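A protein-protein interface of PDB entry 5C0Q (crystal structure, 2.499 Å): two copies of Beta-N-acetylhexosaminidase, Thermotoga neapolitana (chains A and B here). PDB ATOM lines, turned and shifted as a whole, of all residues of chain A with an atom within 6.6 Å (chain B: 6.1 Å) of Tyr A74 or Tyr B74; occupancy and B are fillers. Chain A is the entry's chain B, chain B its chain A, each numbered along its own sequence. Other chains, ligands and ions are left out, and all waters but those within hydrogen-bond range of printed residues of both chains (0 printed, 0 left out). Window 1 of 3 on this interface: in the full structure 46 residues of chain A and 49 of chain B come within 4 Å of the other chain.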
ATOM      1  N   LEU A  39       5.646  -6.969   1.466  1.00  0.00           N
ATOM      2  CA  LEU A  39       5.949  -8.136   0.642  1.00  0.00           C
ATOM      3  C   LEU A  39       4.936  -9.251   0.782  1.00  0.00           C
ATOM      4  O   LEU A  39       4.652  -9.930  -0.165  1.00  0.00           O
ATOM      5  CB  LEU A  39       7.315  -8.657   0.979  1.00  0.00           C
ATOM      6  CG  LEU A  39       8.463  -7.724   0.648  1.00  0.00           C
ATOM      7  CD1 LEU A  39       9.732  -8.174   1.412  1.00  0.00           C
ATOM      8  CD2 LEU A  39       8.709  -7.780  -0.833  1.00  0.00           C
ATOM      9  N   GLU A  42       1.211  -9.320  -2.180  1.00  0.00           N
ATOM     10  CA  GLU A  42       1.785  -9.079  -3.481  1.00  0.00           C
ATOM     11  C   GLU A  42       1.171  -7.879  -4.199  1.00  0.00           C
ATOM     12  O   GLU A  42       1.890  -7.119  -4.851  1.00  0.00           O
ATOM     13  CB  GLU A  42       1.671 -10.303  -4.326  1.00  0.00           C
ATOM     14  CG  GLU A  42       2.329 -10.131  -5.653  1.00  0.00           C
ATOM     15  CD  GLU A  42       2.594 -11.432  -6.294  1.00  0.00           C
ATOM     16  OE1 GLU A  42       1.626 -12.038  -6.743  1.00  0.00           O
ATOM     17  OE2 GLU A  42       3.737 -11.875  -6.325  1.00  0.00           O
ATOM     18  N   PHE A  45       3.023  -4.789  -2.752  1.00  0.00           N
ATOM     19  CA  PHE A  45       4.371  -4.762  -3.268  1.00  0.00           C
ATOM     20  C   PHE A  45       4.435  -4.236  -4.708  1.00  0.00           C
ATOM     21  O   PHE A  45       5.198  -3.311  -5.000  1.00  0.00           O
ATOM     22  CB  PHE A  45       4.962  -6.160  -3.165  1.00  0.00           C
ATOM     23  CG  PHE A  45       6.265  -6.329  -3.861  1.00  0.00           C
ATOM     24  CD1 PHE A  45       7.372  -5.611  -3.465  1.00  0.00           C
ATOM     25  CD2 PHE A  45       6.398  -7.227  -4.908  1.00  0.00           C
ATOM     26  CE1 PHE A  45       8.576  -5.768  -4.119  1.00  0.00           C
ATOM     27  CE2 PHE A  45       7.606  -7.407  -5.544  1.00  0.00           C
ATOM     28  CZ  PHE A  45       8.689  -6.671  -5.172  1.00  0.00           C
ATOM     29  N   LEU A  46       3.594  -4.802  -5.588  1.00  0.00           N
ATOM     30  CA  LEU A  46       3.557  -4.416  -6.970  1.00  0.00           C
ATOM     31  C   LEU A  46       3.115  -2.996  -7.173  1.00  0.00           C
ATOM     32  O   LEU A  46       3.725  -2.278  -7.932  1.00  0.00           O
ATOM     33  CB  LEU A  46       2.666  -5.354  -7.753  1.00  0.00           C
ATOM     34  CG  LEU A  46       3.196  -6.772  -7.816  1.00  0.00           C
ATOM     35  CD1 LEU A  46       2.264  -7.579  -8.564  1.00  0.00           C
ATOM     36  CD2 LEU A  46       4.586  -6.796  -8.415  1.00  0.00           C
ATOM     37  N   HIS A  64      16.746  -9.725   2.508  1.00  0.00           N
ATOM     38  CA  HIS A  64      16.830 -11.112   2.088  1.00  0.00           C
ATOM     39  C   HIS A  64      18.245 -11.667   2.071  1.00  0.00           C
ATOM     40  O   HIS A  64      18.946 -11.597   1.096  1.00  0.00           O
ATOM     41  CB  HIS A  64      16.164 -11.298   0.714  1.00  0.00           C
ATOM     42  CG  HIS A  64      15.854 -12.724   0.414  1.00  0.00           C
ATOM     43  ND1 HIS A  64      14.631 -13.283   0.694  1.00  0.00           N
ATOM     44  CD2 HIS A  64      16.630 -13.722  -0.055  1.00  0.00           C
ATOM     45  CE1 HIS A  64      14.658 -14.563   0.386  1.00  0.00           C
ATOM     46  NE2 HIS A  64      15.861 -14.854  -0.072  1.00  0.00           N
ATOM     47  N   VAL A  71      12.696 -13.027   3.064  1.00  0.00           N
ATOM     48  CA  VAL A  71      11.533 -12.182   2.984  1.00  0.00           C
ATOM     49  C   VAL A  71      10.974 -12.107   1.562  1.00  0.00           C
ATOM     50  O   VAL A  71       9.878 -11.641   1.362  1.00  0.00           O
ATOM     51  CB  VAL A  71      11.815 -10.747   3.479  1.00  0.00           C
ATOM     52  CG1 VAL A  71      12.198 -10.736   4.930  1.00  0.00           C
ATOM     53  CG2 VAL A  71      12.864 -10.022   2.603  1.00  0.00           C
ATOM     54  N   LEU A  72      11.725 -12.578   0.580  1.00  0.00           N
ATOM     55  CA  LEU A  72      11.252 -12.585  -0.774  1.00  0.00           C
ATOM     56  C   LEU A  72      10.874 -14.007  -1.223  1.00  0.00           C
ATOM     57  O   LEU A  72      11.730 -14.837  -1.432  1.00  0.00           O
ATOM     58  CB  LEU A  72      12.306 -12.004  -1.715  1.00  0.00           C
ATOM     59  CG  LEU A  72      12.748 -10.557  -1.525  1.00  0.00           C
ATOM     60  CD1 LEU A  72      13.813 -10.193  -2.528  1.00  0.00           C
ATOM     61  CD2 LEU A  72      11.626  -9.575  -1.555  1.00  0.00           C
ATOM     62  N   LYS A  73       9.589 -14.261  -1.446  1.00  0.00           N
ATOM     63  CA  LYS A  73       9.145 -15.599  -1.877  1.00  0.00           C
ATOM     64  C   LYS A  73       9.702 -15.937  -3.245  1.00  0.00           C
ATOM     65  O   LYS A  73       9.789 -17.099  -3.595  1.00  0.00           O
ATOM     66  CB  LYS A  73       7.618 -15.656  -1.939  1.00  0.00           C
ATOM     67  CG  LYS A  73       7.126 -14.745  -3.093  1.00  0.00           C
ATOM     68  CD  LYS A  73       5.633 -14.631  -3.263  1.00  0.00           C
ATOM     69  CE  LYS A  73       5.015 -15.835  -3.885  1.00  0.00           C
ATOM     70  NZ  LYS A  73       3.575 -15.551  -3.919  1.00  0.00           N
ATOM     71  N   TYR A  74      10.110 -14.911  -3.991  1.00  0.00           N
ATOM     72  CA  TYR A  74      10.655 -15.042  -5.342  1.00  0.00           C
ATOM     73  C   TYR A  74      12.029 -15.673  -5.435  1.00  0.00           C
ATOM     74  O   TYR A  74      12.426 -16.140  -6.487  1.00  0.00           O
ATOM     75  CB  TYR A  74      10.695 -13.661  -6.014  1.00  0.00           C
ATOM     76  CG  TYR A  74       9.413 -12.901  -5.815  1.00  0.00           C
ATOM     77  CD1 TYR A  74       8.229 -13.269  -6.509  1.00  0.00           C
ATOM     78  CD2 TYR A  74       9.353 -11.836  -4.922  1.00  0.00           C
ATOM     79  CE1 TYR A  74       7.064 -12.600  -6.287  1.00  0.00           C
ATOM     80  CE2 TYR A  74       8.185 -11.156  -4.710  1.00  0.00           C
ATOM     81  CZ  TYR A  74       7.049 -11.546  -5.389  1.00  0.00           C
ATOM     82  OH  TYR A  74       5.907 -10.843  -5.165  1.00  0.00           O
ATOM     83  N   VAL A  75      12.768 -15.668  -4.343  1.00  0.00           N
ATOM     84  CA  VAL A  75      14.095 -16.234  -4.328  1.00  0.00           C
ATOM     85  C   VAL A  75      14.008 -17.587  -3.717  1.00  0.00           C
ATOM     86  O   VAL A  75      13.489 -17.715  -2.641  1.00  0.00           O
ATOM     87  CB  VAL A  75      15.077 -15.334  -3.544  1.00  0.00           C
ATOM     88  CG1 VAL A  75      16.435 -15.983  -3.391  1.00  0.00           C
ATOM     89  CG2 VAL A  75      15.172 -14.025  -4.239  1.00  0.00           C
ATOM     90  N   PRO A  76      14.464 -18.615  -4.423  1.00  0.00           N
ATOM     91  CA  PRO A  76      14.378 -19.917  -3.772  1.00  0.00           C
ATOM     92  C   PRO A  76      15.165 -19.908  -2.505  1.00  0.00           C
ATOM     93  O   PRO A  76      16.201 -19.303  -2.459  1.00  0.00           O
ATOM     94  CB  PRO A  76      14.969 -20.889  -4.800  1.00  0.00           C
ATOM     95  CG  PRO A  76      15.682 -20.070  -5.725  1.00  0.00           C
ATOM     96  CD  PRO A  76      15.085 -18.704  -5.738  1.00  0.00           C
ATOM     97  N   SER A  77      14.678 -20.645  -1.537  1.00  0.00           N
ATOM     98  CA  SER A  77      15.212 -20.718  -0.206  1.00  0.00           C
ATOM     99  C   SER A  77      16.599 -21.390  -0.147  1.00  0.00           C
ATOM    100  O   SER A  77      16.904 -22.291  -0.897  1.00  0.00           O
ATOM    101  CB  SER A  77      14.203 -21.458   0.666  1.00  0.00           C
ATOM    102  OG  SER A  77      14.606 -21.499   1.991  1.00  0.00           O
ATOM    103  N   ILE A 102      17.393 -12.255  -9.705  1.00  0.00           N
ATOM    104  CA  ILE A 102      15.998 -12.259  -9.386  1.00  0.00           C
ATOM    105  C   ILE A 102      15.551 -10.962  -8.723  1.00  0.00           C
ATOM    106  O   ILE A 102      14.536 -10.406  -9.119  1.00  0.00           O
ATOM    107  CB  ILE A 102      15.658 -13.436  -8.473  1.00  0.00           C
ATOM    108  CG1 ILE A 102      15.726 -14.756  -9.242  1.00  0.00           C
ATOM    109  CG2 ILE A 102      14.310 -13.261  -7.907  1.00  0.00           C
ATOM    110  CD1 ILE A 102      15.456 -15.950  -8.399  1.00  0.00           C
ATOM    111  N   LEU A 106      12.932  -7.883 -10.201  1.00  0.00           N
ATOM    112  CA  LEU A 106      11.739  -7.363  -9.550  1.00  0.00           C
ATOM    113  C   LEU A 106      11.740  -5.856  -9.368  1.00  0.00           C
ATOM    114  O   LEU A 106      10.680  -5.284  -9.253  1.00  0.00           O
ATOM    115  CB  LEU A 106      11.544  -8.022  -8.179  1.00  0.00           C
ATOM    116  CG  LEU A 106      11.405  -9.535  -8.188  1.00  0.00           C
ATOM    117  CD1 LEU A 106      11.591 -10.103  -6.856  1.00  0.00           C
ATOM    118  CD2 LEU A 106      10.020  -9.862  -8.664  1.00  0.00           C
ATOM    119  N   PHE A 108      14.515  -4.396  -7.221  1.00  0.00           N
ATOM    120  CA  PHE A 108      15.512  -4.087  -6.181  1.00  0.00           C
ATOM    121  C   PHE A 108      16.861  -3.719  -6.796  1.00  0.00           C
ATOM    122  O   PHE A 108      17.231  -4.257  -7.826  1.00  0.00           O
ATOM    123  CB  PHE A 108      15.704  -5.270  -5.227  1.00  0.00           C
ATOM    124  CG  PHE A 108      14.507  -5.581  -4.406  1.00  0.00           C
ATOM    125  CD1 PHE A 108      14.285  -4.935  -3.205  1.00  0.00           C
ATOM    126  CD2 PHE A 108      13.563  -6.499  -4.844  1.00  0.00           C
ATOM    127  CE1 PHE A 108      13.184  -5.214  -2.470  1.00  0.00           C
ATOM    128  CE2 PHE A 108      12.432  -6.776  -4.098  1.00  0.00           C
ATOM    129  CZ  PHE A 108      12.240  -6.140  -2.927  1.00  0.00           C
ATOM    130  N   LEU B  39       7.042 -28.669  -7.957  1.00  0.00           N
ATOM    131  CA  LEU B  39       7.230 -27.260  -7.638  1.00  0.00           C
ATOM    132  C   LEU B  39       6.740 -26.885  -6.241  1.00  0.00           C
ATOM    133  O   LEU B  39       7.322 -26.075  -5.558  1.00  0.00           O
ATOM    134  CB  LEU B  39       6.517 -26.406  -8.678  1.00  0.00           C
ATOM    135  CG  LEU B  39       7.091 -26.601 -10.090  1.00  0.00           C
ATOM    136  CD1 LEU B  39       6.149 -26.067 -11.221  1.00  0.00           C
ATOM    137  CD2 LEU B  39       8.483 -25.972 -10.167  1.00  0.00           C
ATOM    138  N   GLU B  42       9.624 -27.297  -2.667  1.00  0.00           N
ATOM    139  CA  GLU B  42      10.852 -26.664  -3.080  1.00  0.00           C
ATOM    140  C   GLU B  42      12.097 -27.575  -2.899  1.00  0.00           C
ATOM    141  O   GLU B  42      12.972 -27.597  -3.756  1.00  0.00           O
ATOM    142  CB  GLU B  42      11.019 -25.339  -2.368  1.00  0.00           C
ATOM    143  CG  GLU B  42      12.266 -24.630  -2.817  1.00  0.00           C
ATOM    144  CD  GLU B  42      12.208 -23.164  -2.601  1.00  0.00           C
ATOM    145  OE1 GLU B  42      12.739 -22.697  -1.618  1.00  0.00           O
ATOM    146  OE2 GLU B  42      11.620 -22.444  -3.400  1.00  0.00           O
ATOM    147  N   PHE B  45      12.033 -29.722  -5.957  1.00  0.00           N
ATOM    148  CA  PHE B  45      12.356 -28.925  -7.112  1.00  0.00           C
ATOM    149  C   PHE B  45      13.851 -28.677  -7.245  1.00  0.00           C
ATOM    150  O   PHE B  45      14.416 -28.905  -8.315  1.00  0.00           O
ATOM    151  CB  PHE B  45      11.590 -27.605  -7.082  1.00  0.00           C
ATOM    152  CG  PHE B  45      12.019 -26.661  -8.130  1.00  0.00           C
ATOM    153  CD1 PHE B  45      11.887 -27.001  -9.469  1.00  0.00           C
ATOM    154  CD2 PHE B  45      12.591 -25.460  -7.804  1.00  0.00           C
ATOM    155  CE1 PHE B  45      12.298 -26.167 -10.434  1.00  0.00           C
ATOM    156  CE2 PHE B  45      13.013 -24.608  -8.787  1.00  0.00           C
ATOM    157  CZ  PHE B  45      12.875 -24.969 -10.103  1.00  0.00           C
ATOM    158  N   LEU B  46      14.480 -28.236  -6.145  1.00  0.00           N
ATOM    159  CA  LEU B  46      15.898 -27.989  -6.088  1.00  0.00           C
ATOM    160  C   LEU B  46      16.706 -29.243  -6.311  1.00  0.00           C
ATOM    161  O   LEU B  46      17.672 -29.237  -7.048  1.00  0.00           O
ATOM    162  CB  LEU B  46      16.272 -27.385  -4.738  1.00  0.00           C
ATOM    163  CG  LEU B  46      15.625 -26.018  -4.536  1.00  0.00           C
ATOM    164  CD1 LEU B  46      15.918 -25.500  -3.248  1.00  0.00           C
ATOM    165  CD2 LEU B  46      16.033 -25.053  -5.618  1.00  0.00           C
ATOM    166  N   LEU B  72       4.815 -21.202 -10.786  1.00  0.00           N
ATOM    167  CA  LEU B  72       6.082 -20.830 -10.189  1.00  0.00           C
ATOM    168  C   LEU B  72       5.872 -19.718  -9.178  1.00  0.00           C
ATOM    169  O   LEU B  72       5.522 -18.622  -9.526  1.00  0.00           O
ATOM    170  CB  LEU B  72       7.088 -20.399 -11.252  1.00  0.00           C
ATOM    171  CG  LEU B  72       7.533 -21.439 -12.280  1.00  0.00           C
ATOM    172  CD1 LEU B  72       8.484 -20.844 -13.298  1.00  0.00           C
ATOM    173  CD2 LEU B  72       8.113 -22.685 -11.656  1.00  0.00           C
ATOM    174  N   LYS B  73       6.078 -20.000  -7.907  1.00  0.00           N
ATOM    175  CA  LYS B  73       5.895 -18.957  -6.908  1.00  0.00           C
ATOM    176  C   LYS B  73       6.959 -17.845  -7.039  1.00  0.00           C
ATOM    177  O   LYS B  73       6.757 -16.751  -6.556  1.00  0.00           O
ATOM    178  CB  LYS B  73       5.914 -19.535  -5.516  1.00  0.00           C
ATOM    179  CG  LYS B  73       7.249 -20.010  -5.094  1.00  0.00           C
ATOM    180  CD  LYS B  73       7.170 -20.451  -3.652  1.00  0.00           C
ATOM    181  CE  LYS B  73       8.506 -20.751  -3.041  1.00  0.00           C
ATOM    182  NZ  LYS B  73       8.103 -21.292  -1.770  1.00  0.00           N
ATOM    183  N   TYR B  74       8.054 -18.142  -7.728  1.00  0.00           N
ATOM    184  CA  TYR B  74       9.167 -17.237  -7.985  1.00  0.00           C
ATOM    185  C   TYR B  74       8.842 -16.112  -8.970  1.00  0.00           C
ATOM    186  O   TYR B  74       9.572 -15.148  -9.090  1.00  0.00           O
ATOM    187  CB  TYR B  74      10.364 -18.045  -8.504  1.00  0.00           C
ATOM    188  CG  TYR B  74      10.559 -19.331  -7.734  1.00  0.00           C
ATOM    189  CD1 TYR B  74      11.087 -19.326  -6.438  1.00  0.00           C
ATOM    190  CD2 TYR B  74      10.190 -20.545  -8.280  1.00  0.00           C
ATOM    191  CE1 TYR B  74      11.233 -20.500  -5.736  1.00  0.00           C
ATOM    192  CE2 TYR B  74      10.371 -21.706  -7.618  1.00  0.00           C
ATOM    193  CZ  TYR B  74      10.876 -21.688  -6.332  1.00  0.00           C
ATOM    194  OH  TYR B  74      11.035 -22.874  -5.637  1.00  0.00           O
ATOM    195  N   VAL B  75       7.789 -16.273  -9.734  1.00  0.00           N
ATOM    196  CA  VAL B  75       7.368 -15.243 -10.673  1.00  0.00           C
ATOM    197  C   VAL B  75       6.195 -14.462 -10.129  1.00  0.00           C
ATOM    198  O   VAL B  75       5.199 -15.025  -9.772  1.00  0.00           O
ATOM    199  CB  VAL B  75       7.014 -15.871 -12.032  1.00  0.00           C
ATOM    200  CG1 VAL B  75       6.413 -14.880 -12.983  1.00  0.00           C
ATOM    201  CG2 VAL B  75       8.244 -16.499 -12.620  1.00  0.00           C
ATOM    202  N   PRO B  76       6.315 -13.155 -10.051  1.00  0.00           N
ATOM    203  CA  PRO B  76       5.158 -12.424  -9.548  1.00  0.00           C
ATOM    204  C   PRO B  76       3.913 -12.692 -10.381  1.00  0.00           C
ATOM    205  O   PRO B  76       3.998 -12.790 -11.587  1.00  0.00           O
ATOM    206  CB  PRO B  76       5.570 -10.971  -9.686  1.00  0.00           C
ATOM    207  CG  PRO B  76       6.960 -11.004  -9.812  1.00  0.00           C
ATOM    208  CD  PRO B  76       7.384 -12.257 -10.449  1.00  0.00           C
ATOM    209  N   SER B  77       2.776 -12.729  -9.713  1.00  0.00           N
ATOM    210  CA  SER B  77       1.497 -13.064 -10.288  1.00  0.00           C
ATOM    211  C   SER B  77       0.985 -11.956 -11.232  1.00  0.00           C
ATOM    212  O   SER B  77       1.118 -10.774 -10.944  1.00  0.00           O
ATOM    213  CB  SER B  77       0.507 -13.340  -9.154  1.00  0.00           C
ATOM    214  OG  SER B  77      -0.732 -13.757  -9.631  1.00  0.00           O
ATOM    215  N   ILE B 102      13.512 -14.495 -14.621  1.00  0.00           N
ATOM    216  CA  ILE B 102      13.380 -15.240 -13.385  1.00  0.00           C
ATOM    217  C   ILE B 102      13.428 -16.738 -13.631  1.00  0.00           C
ATOM    218  O   ILE B 102      14.143 -17.451 -12.937  1.00  0.00           O
ATOM    219  CB  ILE B 102      12.089 -14.847 -12.654  1.00  0.00           C
ATOM    220  CG1 ILE B 102      12.229 -13.440 -12.100  1.00  0.00           C
ATOM    221  CG2 ILE B 102      11.822 -15.792 -11.545  1.00  0.00           C
ATOM    222  CD1 ILE B 102      11.007 -12.914 -11.493  1.00  0.00           C
ATOM    223  N   LEU B 106      16.330 -19.605 -12.544  1.00  0.00           N
ATOM    224  CA  LEU B 106      16.086 -20.854 -11.825  1.00  0.00           C
ATOM    225  C   LEU B 106      16.590 -22.103 -12.538  1.00  0.00           C
ATOM    226  O   LEU B 106      16.811 -23.106 -11.895  1.00  0.00           O
ATOM    227  CB  LEU B 106      14.607 -21.016 -11.542  1.00  0.00           C
ATOM    228  CG  LEU B 106      14.048 -19.859 -10.732  1.00  0.00           C
ATOM    229  CD1 LEU B 106      12.594 -19.912 -10.743  1.00  0.00           C
ATOM    230  CD2 LEU B 106      14.571 -19.871  -9.329  1.00  0.00           C
ATOM    231  N   PHE B 108      15.134 -22.965 -15.893  1.00  0.00           N
ATOM    232  CA  PHE B 108      14.258 -23.213 -17.029  1.00  0.00           C
ATOM    233  C   PHE B 108      14.848 -22.630 -18.303  1.00  0.00           C
ATOM    234  O   PHE B 108      15.510 -21.576 -18.270  1.00  0.00           O
ATOM    235  CB  PHE B 108      12.879 -22.609 -16.782  1.00  0.00           C
ATOM    236  CG  PHE B 108      12.115 -23.287 -15.713  1.00  0.00           C
ATOM    237  CD1 PHE B 108      11.376 -24.410 -15.992  1.00  0.00           C
ATOM    238  CD2 PHE B 108      12.127 -22.809 -14.408  1.00  0.00           C
ATOM    239  CE1 PHE B 108      10.654 -25.038 -14.997  1.00  0.00           C
ATOM    240  CE2 PHE B 108      11.415 -23.450 -13.411  1.00  0.00           C
ATOM    241  CZ  PHE B 108      10.690 -24.561 -13.704  1.00  0.00           C
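Tyr B74 touches just these residues of chain A: Lys A73, Tyr A74 and Pro A76.
Printed residues of chain A within 4 Å of Leu B106: Pro A76.
Printed residues of chain B within 4 Å of Pro A76: Glu B42, Tyr B74 and Leu B106.
The nearest residue of chain B that does not touch Tyr A74 is Val B75 (4.3 Å).
OE2 of Glu A42 lies within hydrogen-bond range of OH of Tyr A74, at 2.7 Å.
Of the 13 printed residues of chain B, 6 touch a printed residue of chain A.
Of the 15 printed residues of chain A, 6 touch a printed residue of chain B.
Pro B76 touches Glu A42 (CA to OE2, 3.6 Å).
CE of Lys A73 touches O of Lys B73, 3.3 Å away.
Lys A73 touches Tyr B74 (O to CD1, 3.8 Å).
Tyr A74 touches Lys B73 (CD1 to O, 3.8 Å).
Tyr B74 touches Tyr A74 (CD1 to O, 3.5 Å).
Pro B76 touches Tyr A74 (CA to CE1, 3.8 Å).
OE2 of Glu B42 touches CA of Pro A76, 3.8 Å away.
CA of Pro A76 touches CE1 of Tyr B74, 3.8 Å away.
Pro A76 touches Leu B106.
Pro B76 touches Leu A106 (CG to CD2, 3.5 Å).
Glu A42 touches Pro B76, and with the chains exchanged Pro A76 touches Glu B42.
Lys A73 touches its own counterpart, Lys B73.
Lys A73 touches Tyr B74, and with the chains exchanged Tyr A74 touches Lys B73.
Tyr A74 touches Pro B76, and with the chains exchanged Pro A76 touches Tyr B74.
Positions printed for both chains: 39, 42, 45, 46, 72, 73, 74, 75, 76, 77, 102, 106 and 108.
The backbone NH (N) of Ser B77 sits close to the side-chain carboxylate (OE1) of Glu A42 (3.3 Å).
OE1 of Glu B42 is in hydrogen-bond range of N of Ser A77, 2.8 Å away.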
